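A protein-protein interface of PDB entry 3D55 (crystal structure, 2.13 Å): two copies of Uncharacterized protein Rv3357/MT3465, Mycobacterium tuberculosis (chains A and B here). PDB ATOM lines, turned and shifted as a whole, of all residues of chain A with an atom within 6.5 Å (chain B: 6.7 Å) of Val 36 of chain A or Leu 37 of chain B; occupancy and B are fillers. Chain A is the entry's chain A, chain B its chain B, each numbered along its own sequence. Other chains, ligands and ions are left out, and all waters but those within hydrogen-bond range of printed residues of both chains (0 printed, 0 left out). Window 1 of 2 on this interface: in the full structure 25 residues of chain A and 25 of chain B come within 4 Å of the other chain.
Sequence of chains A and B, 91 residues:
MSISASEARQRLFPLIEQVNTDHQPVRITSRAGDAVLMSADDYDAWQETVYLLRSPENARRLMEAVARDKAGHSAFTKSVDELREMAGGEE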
ATOM      1  N   PRO A  25      27.257  -7.993 -18.074  1.00  0.00           N
ATOM      2  CA  PRO A  25      26.944  -7.083 -19.184  1.00  0.00           C
ATOM      3  C   PRO A  25      25.628  -7.504 -19.917  1.00  0.00           C
ATOM      4  O   PRO A  25      25.122  -8.638 -19.744  1.00  0.00           O
ATOM      5  CB  PRO A  25      28.142  -7.219 -20.066  1.00  0.00           C
ATOM      6  CG  PRO A  25      28.430  -8.941 -19.951  1.00  0.00           C
ATOM      7  CD  PRO A  25      28.292  -9.046 -18.418  1.00  0.00           C
ATOM      8  N   VAL A  26      25.058  -6.591 -20.713  1.00  0.00           N
ATOM      9  CA  VAL A  26      23.860  -6.931 -21.506  1.00  0.00           C
ATOM     10  C   VAL A  26      24.218  -6.857 -22.959  1.00  0.00           C
ATOM     11  O   VAL A  26      24.586  -5.749 -23.409  1.00  0.00           O
ATOM     12  CB  VAL A  26      22.688  -5.951 -21.295  1.00  0.00           C
ATOM     13  CG1 VAL A  26      21.530  -6.450 -22.079  1.00  0.00           C
ATOM     14  CG2 VAL A  26      22.318  -5.857 -19.828  1.00  0.00           C
ATOM     15  N   ARG A  27      24.121  -8.005 -23.641  1.00  0.00           N
ATOM     16  CA  ARG A  27      24.265  -8.151 -25.111  1.00  0.00           C
ATOM     17  C   ARG A  27      22.993  -7.756 -25.856  1.00  0.00           C
ATOM     18  O   ARG A  27      21.904  -8.324 -25.626  1.00  0.00           O
ATOM     19  CB  ARG A  27      24.516  -9.602 -25.480  1.00  0.00           C
ATOM     20  CG  ARG A  27      25.796 -10.150 -24.972  1.00  0.00           C
ATOM     21  CD  ARG A  27      26.802 -10.383 -26.088  1.00  0.00           C
ATOM     22  NE  ARG A  27      28.022 -10.826 -25.438  1.00  0.00           N
ATOM     23  CZ  ARG A  27      29.133 -11.274 -26.015  1.00  0.00           C
ATOM     24  NH1 ARG A  27      29.270 -11.361 -27.348  1.00  0.00           N
ATOM     25  NH2 ARG A  27      30.127 -11.618 -25.208  1.00  0.00           N
ATOM     26  N   ILE A  28      23.145  -6.738 -26.698  1.00  0.00           N
ATOM     27  CA  ILE A  28      22.060  -6.205 -27.497  1.00  0.00           C
ATOM     28  C   ILE A  28      22.329  -6.592 -28.949  1.00  0.00           C
ATOM     29  O   ILE A  28      23.399  -6.247 -29.526  1.00  0.00           O
ATOM     30  CB  ILE A  28      22.003  -4.674 -27.420  1.00  0.00           C
ATOM     31  CG1 ILE A  28      21.688  -4.247 -25.999  1.00  0.00           C
ATOM     32  CG2 ILE A  28      20.942  -4.144 -28.426  1.00  0.00           C
ATOM     33  CD1 ILE A  28      21.997  -2.829 -25.680  1.00  0.00           C
ATOM     34  N   ASP A  34      26.184  -5.950 -32.978  1.00  0.00           N
ATOM     35  CA  ASP A  34      25.815  -6.250 -31.628  1.00  0.00           C
ATOM     36  C   ASP A  34      26.547  -5.226 -30.749  1.00  0.00           C
ATOM     37  O   ASP A  34      27.604  -4.658 -31.128  1.00  0.00           O
ATOM     38  CB  ASP A  34      26.183  -7.709 -31.268  1.00  0.00           C
ATOM     39  CG  ASP A  34      25.469  -8.763 -32.178  1.00  0.00           C
ATOM     40  OD1 ASP A  34      24.267  -8.630 -32.416  1.00  0.00           O
ATOM     41  OD2 ASP A  34      26.112  -9.732 -32.668  1.00  0.00           O
ATOM     42  N   ALA A  35      25.986  -4.981 -29.571  1.00  0.00           N
ATOM     43  CA  ALA A  35      26.597  -4.063 -28.651  1.00  0.00           C
ATOM     44  C   ALA A  35      26.439  -4.678 -27.270  1.00  0.00           C
ATOM     45  O   ALA A  35      25.624  -5.539 -27.106  1.00  0.00           O
ATOM     46  CB  ALA A  35      25.957  -2.707 -28.762  1.00  0.00           C
ATOM     47  N   VAL A  36      27.327  -4.320 -26.347  1.00  0.00           N
ATOM     48  CA  VAL A  36      27.224  -4.660 -24.913  1.00  0.00           C
ATOM     49  C   VAL A  36      26.945  -3.379 -24.078  1.00  0.00           C
ATOM     50  O   VAL A  36      27.535  -2.388 -24.337  1.00  0.00           O
ATOM     51  CB  VAL A  36      28.493  -5.383 -24.432  1.00  0.00           C
ATOM     52  CG1 VAL A  36      28.530  -5.441 -22.847  1.00  0.00           C
ATOM     53  CG2 VAL A  36      28.584  -6.810 -25.102  1.00  0.00           C
ATOM     54  N   LEU A  37      26.043  -3.470 -23.128  1.00  0.00           N
ATOM     55  CA  LEU A  37      25.696  -2.395 -22.239  1.00  0.00           C
ATOM     56  C   LEU A  37      26.299  -2.893 -20.966  1.00  0.00           C
ATOM     57  O   LEU A  37      25.974  -4.033 -20.560  1.00  0.00           O
ATOM     58  CB  LEU A  37      24.115  -2.298 -22.079  1.00  0.00           C
ATOM     59  CG  LEU A  37      23.879  -1.079 -21.097  1.00  0.00           C
ATOM     60  CD1 LEU A  37      24.482   0.229 -21.693  1.00  0.00           C
ATOM     61  CD2 LEU A  37      22.431  -0.861 -20.649  1.00  0.00           C
ATOM     62  N   MET A  38      27.251  -2.163 -20.369  1.00  0.00           N
ATOM     63  CA  MET A  38      27.743  -2.532 -19.026  1.00  0.00           C
ATOM     64  C   MET A  38      27.798  -1.356 -18.047  1.00  0.00           C
ATOM     65  O   MET A  38      27.720  -0.218 -18.460  1.00  0.00           O
ATOM     66  CB  MET A  38      29.190  -3.027 -19.090  1.00  0.00           C
ATOM     67  CG  MET A  38      30.093  -1.997 -19.743  1.00  0.00           C
ATOM     68  SD  MET A  38      31.775  -2.651 -20.202  1.00  0.00           S
ATOM     69  CE  MET A  38      32.278  -3.267 -18.595  1.00  0.00           C
ATOM     70  N   LEU B  12      19.100   5.040 -29.742  1.00  0.00           N
ATOM     71  CA  LEU B  12      19.803   3.757 -29.478  1.00  0.00           C
ATOM     72  C   LEU B  12      20.382   3.162 -30.751  1.00  0.00           C
ATOM     73  O   LEU B  12      21.593   2.899 -30.846  1.00  0.00           O
ATOM     74  CB  LEU B  12      18.921   2.730 -28.734  1.00  0.00           C
ATOM     75  CG  LEU B  12      19.814   1.564 -28.306  1.00  0.00           C
ATOM     76  CD1 LEU B  12      20.921   2.074 -27.317  1.00  0.00           C
ATOM     77  CD2 LEU B  12      19.065   0.382 -27.762  1.00  0.00           C
ATOM     78  N   LEU B  15      23.124   5.013 -32.114  1.00  0.00           N
ATOM     79  CA  LEU B  15      24.233   4.797 -31.154  1.00  0.00           C
ATOM     80  C   LEU B  15      24.867   3.402 -31.379  1.00  0.00           C
ATOM     81  O   LEU B  15      26.092   3.289 -31.396  1.00  0.00           O
ATOM     82  CB  LEU B  15      23.752   4.921 -29.700  1.00  0.00           C
ATOM     83  CG  LEU B  15      23.524   6.339 -29.198  1.00  0.00           C
ATOM     84  CD1 LEU B  15      23.093   6.274 -27.723  1.00  0.00           C
ATOM     85  CD2 LEU B  15      24.737   7.235 -29.440  1.00  0.00           C
ATOM     86  N   ILE B  16      24.031   2.369 -31.594  1.00  0.00           N
ATOM     87  CA  ILE B  16      24.493   0.990 -31.853  1.00  0.00           C
ATOM     88  C   ILE B  16      25.363   0.831 -33.123  1.00  0.00           C
ATOM     89  O   ILE B  16      26.368   0.124 -33.097  1.00  0.00           O
ATOM     90  CB  ILE B  16      23.357  -0.021 -31.912  1.00  0.00           C
ATOM     91  CG1 ILE B  16      22.923  -0.444 -30.519  1.00  0.00           C
ATOM     92  CG2 ILE B  16      23.816  -1.391 -32.590  1.00  0.00           C
ATOM     93  CD1 ILE B  16      21.550  -0.916 -30.418  1.00  0.00           C
ATOM     94  N   VAL B  19      28.731   2.798 -32.375  1.00  0.00           N
ATOM     95  CA  VAL B  19      29.653   2.036 -31.541  1.00  0.00           C
ATOM     96  C   VAL B  19      30.358   0.913 -32.374  1.00  0.00           C
ATOM     97  O   VAL B  19      31.505   0.571 -32.120  1.00  0.00           O
ATOM     98  CB  VAL B  19      28.867   1.581 -30.310  1.00  0.00           C
ATOM     99  CG1 VAL B  19      28.746   0.164 -30.227  1.00  0.00           C
ATOM    100  CG2 VAL B  19      29.267   2.377 -29.047  1.00  0.00           C
ATOM    101  N   GLN B  24      34.166   3.364 -30.893  1.00  0.00           N
ATOM    102  CA  GLN B  24      34.395   4.103 -29.637  1.00  0.00           C
ATOM    103  C   GLN B  24      33.223   3.977 -28.648  1.00  0.00           C
ATOM    104  O   GLN B  24      32.123   4.369 -28.978  1.00  0.00           O
ATOM    105  CB  GLN B  24      34.699   5.593 -29.893  1.00  0.00           C
ATOM    106  CG  GLN B  24      35.731   5.781 -30.930  1.00  0.00           C
ATOM    107  CD  GLN B  24      36.050   7.245 -31.251  1.00  0.00           C
ATOM    108  OE1 GLN B  24      35.668   8.172 -30.521  1.00  0.00           O
ATOM    109  NE2 GLN B  24      36.761   7.451 -32.359  1.00  0.00           N
ATOM    110  N   PRO B  25      33.488   3.525 -27.405  1.00  0.00           N
ATOM    111  CA  PRO B  25      32.440   3.337 -26.386  1.00  0.00           C
ATOM    112  C   PRO B  25      31.725   4.685 -26.016  1.00  0.00           C
ATOM    113  O   PRO B  25      32.359   5.702 -25.985  1.00  0.00           O
ATOM    114  CB  PRO B  25      33.198   2.759 -25.200  1.00  0.00           C
ATOM    115  CG  PRO B  25      34.572   2.306 -25.773  1.00  0.00           C
ATOM    116  CD  PRO B  25      34.836   3.388 -26.814  1.00  0.00           C
ATOM    117  N   VAL B  26      30.420   4.676 -25.781  1.00  0.00           N
ATOM    118  CA  VAL B  26      29.702   5.934 -25.412  1.00  0.00           C
ATOM    119  C   VAL B  26      29.259   5.848 -23.939  1.00  0.00           C
ATOM    120  O   VAL B  26      28.841   4.785 -23.448  1.00  0.00           O
ATOM    121  CB  VAL B  26      28.467   6.113 -26.278  1.00  0.00           C
ATOM    122  CG1 VAL B  26      27.567   7.289 -25.764  1.00  0.00           C
ATOM    123  CG2 VAL B  26      28.893   6.332 -27.746  1.00  0.00           C
ATOM    124  N   ARG B  27      29.356   6.963 -23.248  1.00  0.00           N
ATOM    125  CA  ARG B  27      29.160   6.939 -21.816  1.00  0.00           C
ATOM    126  C   ARG B  27      27.768   7.504 -21.606  1.00  0.00           C
ATOM    127  O   ARG B  27      27.387   8.455 -22.278  1.00  0.00           O
ATOM    128  CB  ARG B  27      30.273   7.743 -21.122  1.00  0.00           C
ATOM    129  CG  ARG B  27      30.337   7.525 -19.585  1.00  0.00           C
ATOM    130  CD  ARG B  27      31.457   8.397 -18.903  1.00  0.00           C
ATOM    131  NE  ARG B  27      32.808   7.940 -19.246  1.00  0.00           N
ATOM    132  CZ  ARG B  27      33.448   6.920 -18.658  1.00  0.00           C
ATOM    133  NH1 ARG B  27      32.873   6.237 -17.686  1.00  0.00           N
ATOM    134  NH2 ARG B  27      34.669   6.605 -19.047  1.00  0.00           N
ATOM    135  N   ILE B  28      26.993   6.845 -20.750  1.00  0.00           N
ATOM    136  CA  ILE B  28      25.594   7.213 -20.474  1.00  0.00           C
ATOM    137  C   ILE B  28      25.410   7.491 -18.989  1.00  0.00           C
ATOM    138  O   ILE B  28      25.718   6.662 -18.084  1.00  0.00           O
ATOM    139  CB  ILE B  28      24.657   6.163 -20.966  1.00  0.00           C
ATOM    140  CG1 ILE B  28      24.905   5.903 -22.448  1.00  0.00           C
ATOM    141  CG2 ILE B  28      23.156   6.573 -20.879  1.00  0.00           C
ATOM    142  CD1 ILE B  28      24.487   4.515 -22.879  1.00  0.00           C
ATOM    143  N   ALA B  35      26.316   4.111 -17.394  1.00  0.00           N
ATOM    144  CA  ALA B  35      26.560   2.878 -18.229  1.00  0.00           C
ATOM    145  C   ALA B  35      27.545   3.224 -19.319  1.00  0.00           C
ATOM    146  O   ALA B  35      27.825   4.443 -19.580  1.00  0.00           O
ATOM    147  CB  ALA B  35      25.267   2.347 -18.855  1.00  0.00           C
ATOM    148  N   VAL B  36      28.049   2.198 -19.974  1.00  0.00           N
ATOM    149  CA  VAL B  36      28.862   2.408 -21.204  1.00  0.00           C
ATOM    150  C   VAL B  36      28.289   1.449 -22.190  1.00  0.00           C
ATOM    151  O   VAL B  36      27.941   0.314 -21.832  1.00  0.00           O
ATOM    152  CB  VAL B  36      30.398   2.153 -20.958  1.00  0.00           C
ATOM    153  CG1 VAL B  36      31.132   2.304 -22.255  1.00  0.00           C
ATOM    154  CG2 VAL B  36      30.976   3.230 -19.994  1.00  0.00           C
ATOM    155  N   LEU B  37      28.117   1.906 -23.399  1.00  0.00           N
ATOM    156  CA  LEU B  37      27.631   1.110 -24.437  1.00  0.00           C
ATOM    157  C   LEU B  37      28.816   1.049 -25.385  1.00  0.00           C
ATOM    158  O   LEU B  37      29.343   2.101 -25.716  1.00  0.00           O
ATOM    159  CB  LEU B  37      26.422   1.790 -25.137  1.00  0.00           C
ATOM    160  CG  LEU B  37      25.940   1.035 -26.311  1.00  0.00           C
ATOM    161  CD1 LEU B  37      25.109  -0.305 -25.881  1.00  0.00           C
ATOM    162  CD2 LEU B  37      25.156   2.028 -27.331  1.00  0.00           C
ATOM    163  N   MET B  38      29.162  -0.142 -25.892  1.00  0.00           N
ATOM    164  CA  MET B  38      30.307  -0.353 -26.797  1.00  0.00           C
ATOM    165  C   MET B  38      30.070  -1.523 -27.766  1.00  0.00           C
ATOM    166  O   MET B  38      29.066  -2.250 -27.629  1.00  0.00           O
ATOM    167  CB  MET B  38      31.566  -0.678 -25.938  1.00  0.00           C
ATOM    168  CG  MET B  38      31.443  -1.994 -25.157  1.00  0.00           C
ATOM    169  SD  MET B  38      32.906  -2.214 -23.989  1.00  0.00           S
ATOM    170  CE  MET B  38      34.276  -2.265 -25.011  1.00  0.00           C
ATOM    171  N   SER B  39      30.944  -1.752 -28.753  1.00  0.00           N
ATOM    172  CA  SER B  39      30.519  -2.870 -29.631  1.00  0.00           C
ATOM    173  C   SER B  39      30.715  -4.184 -28.902  1.00  0.00           C
ATOM    174  O   SER B  39      31.565  -4.258 -28.000  1.00  0.00           O
ATOM    175  CB  SER B  39      31.239  -2.904 -30.951  1.00  0.00           C
ATOM    176  OG  SER B  39      32.579  -3.120 -30.712  1.00  0.00           O
ATOM    177  N   ALA B  40      29.928  -5.191 -29.299  1.00  0.00           N
ATOM    178  CA  ALA B  40      30.084  -6.510 -28.680  1.00  0.00           C
ATOM    179  C   ALA B  40      31.472  -6.953 -29.022  1.00  0.00           C
ATOM    180  O   ALA B  40      32.123  -7.633 -28.267  1.00  0.00           O
ATOM    181  CB  ALA B  40      29.017  -7.673 -29.271  1.00  0.00           C
ATOM    182  N   ASP B  41      31.921  -6.554 -30.179  1.00  0.00           N
ATOM    183  CA  ASP B  41      33.279  -7.048 -30.615  1.00  0.00           C
ATOM    184  C   ASP B  41      34.439  -6.472 -29.774  1.00  0.00           C
ATOM    185  O   ASP B  41      35.380  -7.212 -29.430  1.00  0.00           O
ATOM    186  CB  ASP B  41      33.506  -6.850 -32.086  1.00  0.00           C
ATOM    187  CG  ASP B  41      32.648  -7.809 -32.965  1.00  0.00           C
ATOM    188  OD1 ASP B  41      32.002  -8.741 -32.457  1.00  0.00           O
ATOM    189  OD2 ASP B  41      32.663  -7.635 -34.195  1.00  0.00           O
ATOM    190  N   TYR B  43      34.167  -5.617 -26.762  1.00  0.00           N
ATOM    191  CA  TYR B  43      34.003  -6.155 -25.417  1.00  0.00           C
ATOM    192  C   TYR B  43      34.524  -7.616 -25.409  1.00  0.00           C
ATOM    193  O   TYR B  43      35.392  -7.944 -24.578  1.00  0.00           O
ATOM    194  CB  TYR B  43      32.586  -6.173 -25.053  1.00  0.00           C
ATOM    195  CG  TYR B  43      32.387  -6.731 -23.656  1.00  0.00           C
ATOM    196  CD1 TYR B  43      32.355  -5.855 -22.564  1.00  0.00           C
ATOM    197  CD2 TYR B  43      32.104  -8.113 -23.431  1.00  0.00           C
ATOM    198  CE1 TYR B  43      32.114  -6.317 -21.254  1.00  0.00           C
ATOM    199  CE2 TYR B  43      31.883  -8.577 -22.150  1.00  0.00           C
ATOM    200  CZ  TYR B  43      31.922  -7.652 -21.056  1.00  0.00           C
ATOM    201  OH  TYR B  43      31.697  -8.012 -19.778  1.00  0.00           O
ATOM    202  N   ASP B  44      34.076  -8.410 -26.422  1.00  0.00           N
ATOM    203  CA  ASP B  44      34.564  -9.803 -26.526  1.00  0.00           C
ATOM    204  C   ASP B  44      36.112  -9.853 -26.686  1.00  0.00           C
ATOM    205  O   ASP B  44      36.755 -10.693 -26.118  1.00  0.00           O
ATOM    206  CB  ASP B  44      33.983 -10.438 -27.754  1.00  0.00           C
ATOM    207  CG  ASP B  44      32.516 -10.719 -27.569  1.00  0.00           C
ATOM    208  OD1 ASP B  44      32.027 -10.729 -26.395  1.00  0.00           O
ATOM    209  OD2 ASP B  44      31.914 -11.085 -28.590  1.00  0.00           O
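The guanidinium group (NH2) of Arg 27 of chain A is in salt-bridge range of the side-chain carboxylate (OD1) of Asp 44 of chain B. The backbone NH (N) of Val 36 of chain A is in hydrogen-bond range of the backbone carbonyl oxygen (O) of Met 38 of chain B (3.0 Å). O of Met 38 of chain A sits at hydrogen-bond distance from N of Val 36 of chain B, at 2.9 Å. O of Asp 34 of chain A sits at hydrogen-bond distance from N of Ala 40 of chain B (3.0 Å).
O of Ile 28 of chain B is in hydrogen-bond range of N of Ala 35 of chain B, at 2.7 Å. O of Val 26 of chain A lies within hydrogen-bond range of N of Leu 37 of chain A. The backbone carbonyl oxygen of Ala 35 of chain A is in hydrogen-bond range of the backbone NH of Ile 28 of chain A. N of Val 26 of chain B sits at hydrogen-bond distance from O of Leu 37 of chain B.
Among the printed residues, merely in contact across the chains: Ala 35 of chain A with Met 38 of chain B (3.2 Å), Met 38 of chain A with Ala 35 of chain B (3.3 Å), Pro 25 of chain A with Tyr 43 of chain B (3.4 Å), Leu 37 of chain A with Val 36 of chain B (3.5 Å), Val 36 of chain A with Leu 37 of chain B (3.5 Å), Ala 35 of chain A with Ala 40 of chain B (3.6 Å), Leu 37 of chain A with Ala 35 of chain B (3.6 Å), Val 36 of chain A with Val 36 of chain B (3.7 Å), Asp 34 of chain A with Ser 39 of chain B (3.7 Å), Met 38 of chain A with Tyr 43 of chain B (3.8 Å), Ile 28 of chain A with Ile 16 of chain B (3.8 Å), Ala 35 of chain A with Leu 37 of chain B (3.8 Å), Val 36 of chain A with Tyr 43 of chain B (3.9 Å), Val 36 of chain A with Ala 40 of chain B (3.9 Å) and Met 38 of chain A with Met 38 of chain B (3.98 Å).
Of chain B, only Val 36 (3.7 Å), Leu 37 (3.5 Å), Met 38 (3.0 Å), Ala 40 (3.9 Å) and Tyr 43 (3.9 Å) come within 4 Å of Val 36 of chain A. Of the printed residues of chain A, Leu 37 of chain B touches Ala 35 and Val 36. Printed residues of chain B within 4 Å of Arg 27 of chain A: Asp 44. Of the printed residues of chain A, Asp 44 of chain B touches Arg 27. Arg 27 of chain B touches none of the printed residues of chain A. Leu 12 of chain B touches none of the printed residues of chain A. The nearest printed residue of chain B that does not touch Arg 27 of chain A is Ala 40 of chain B (4.2 Å).
Of the 9 printed residues of chain A, 8 touch a printed residue of chain B. Along chain A the printed residues that touch a printed residue of chain B span positions 25 to 38. Hydrophobic or aromatic side chains of chain B within 4 Å of the printed part of chain A: Ile 16, Ala 35, Leu 37, Met 38, Ala 40 and Tyr 43. Among the printed residues, 19 pairs touch across the chains. Among the printed residues, Asp or Glu carboxylates within 4 Å of a Lys or Arg side-chain nitrogen of the other chain: Arg 27 of chain A with Asp 44 of chain B (2.4 Å).
Ala 35 of chain A touches Leu 37 of chain B, and with the chains exchanged Leu 37 of chain A touches Ala 35 of chain B. Ala 35 of chain A touches Met 38 of chain B, and with the chains exchanged Met 38 of chain A touches Ala 35 of chain B. Val 36 of chain A touches Met 38 of chain B, and with the chains exchanged Met 38 of chain A touches Val 36 of chain B. Met 38 of chain B touches its own counterpart, Met 38 of chain A. 8 positions are printed for both chains. Of the 19 pairs that touch across the chains among the printed residues, 10 have their exchanged pair printed and touching as well.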
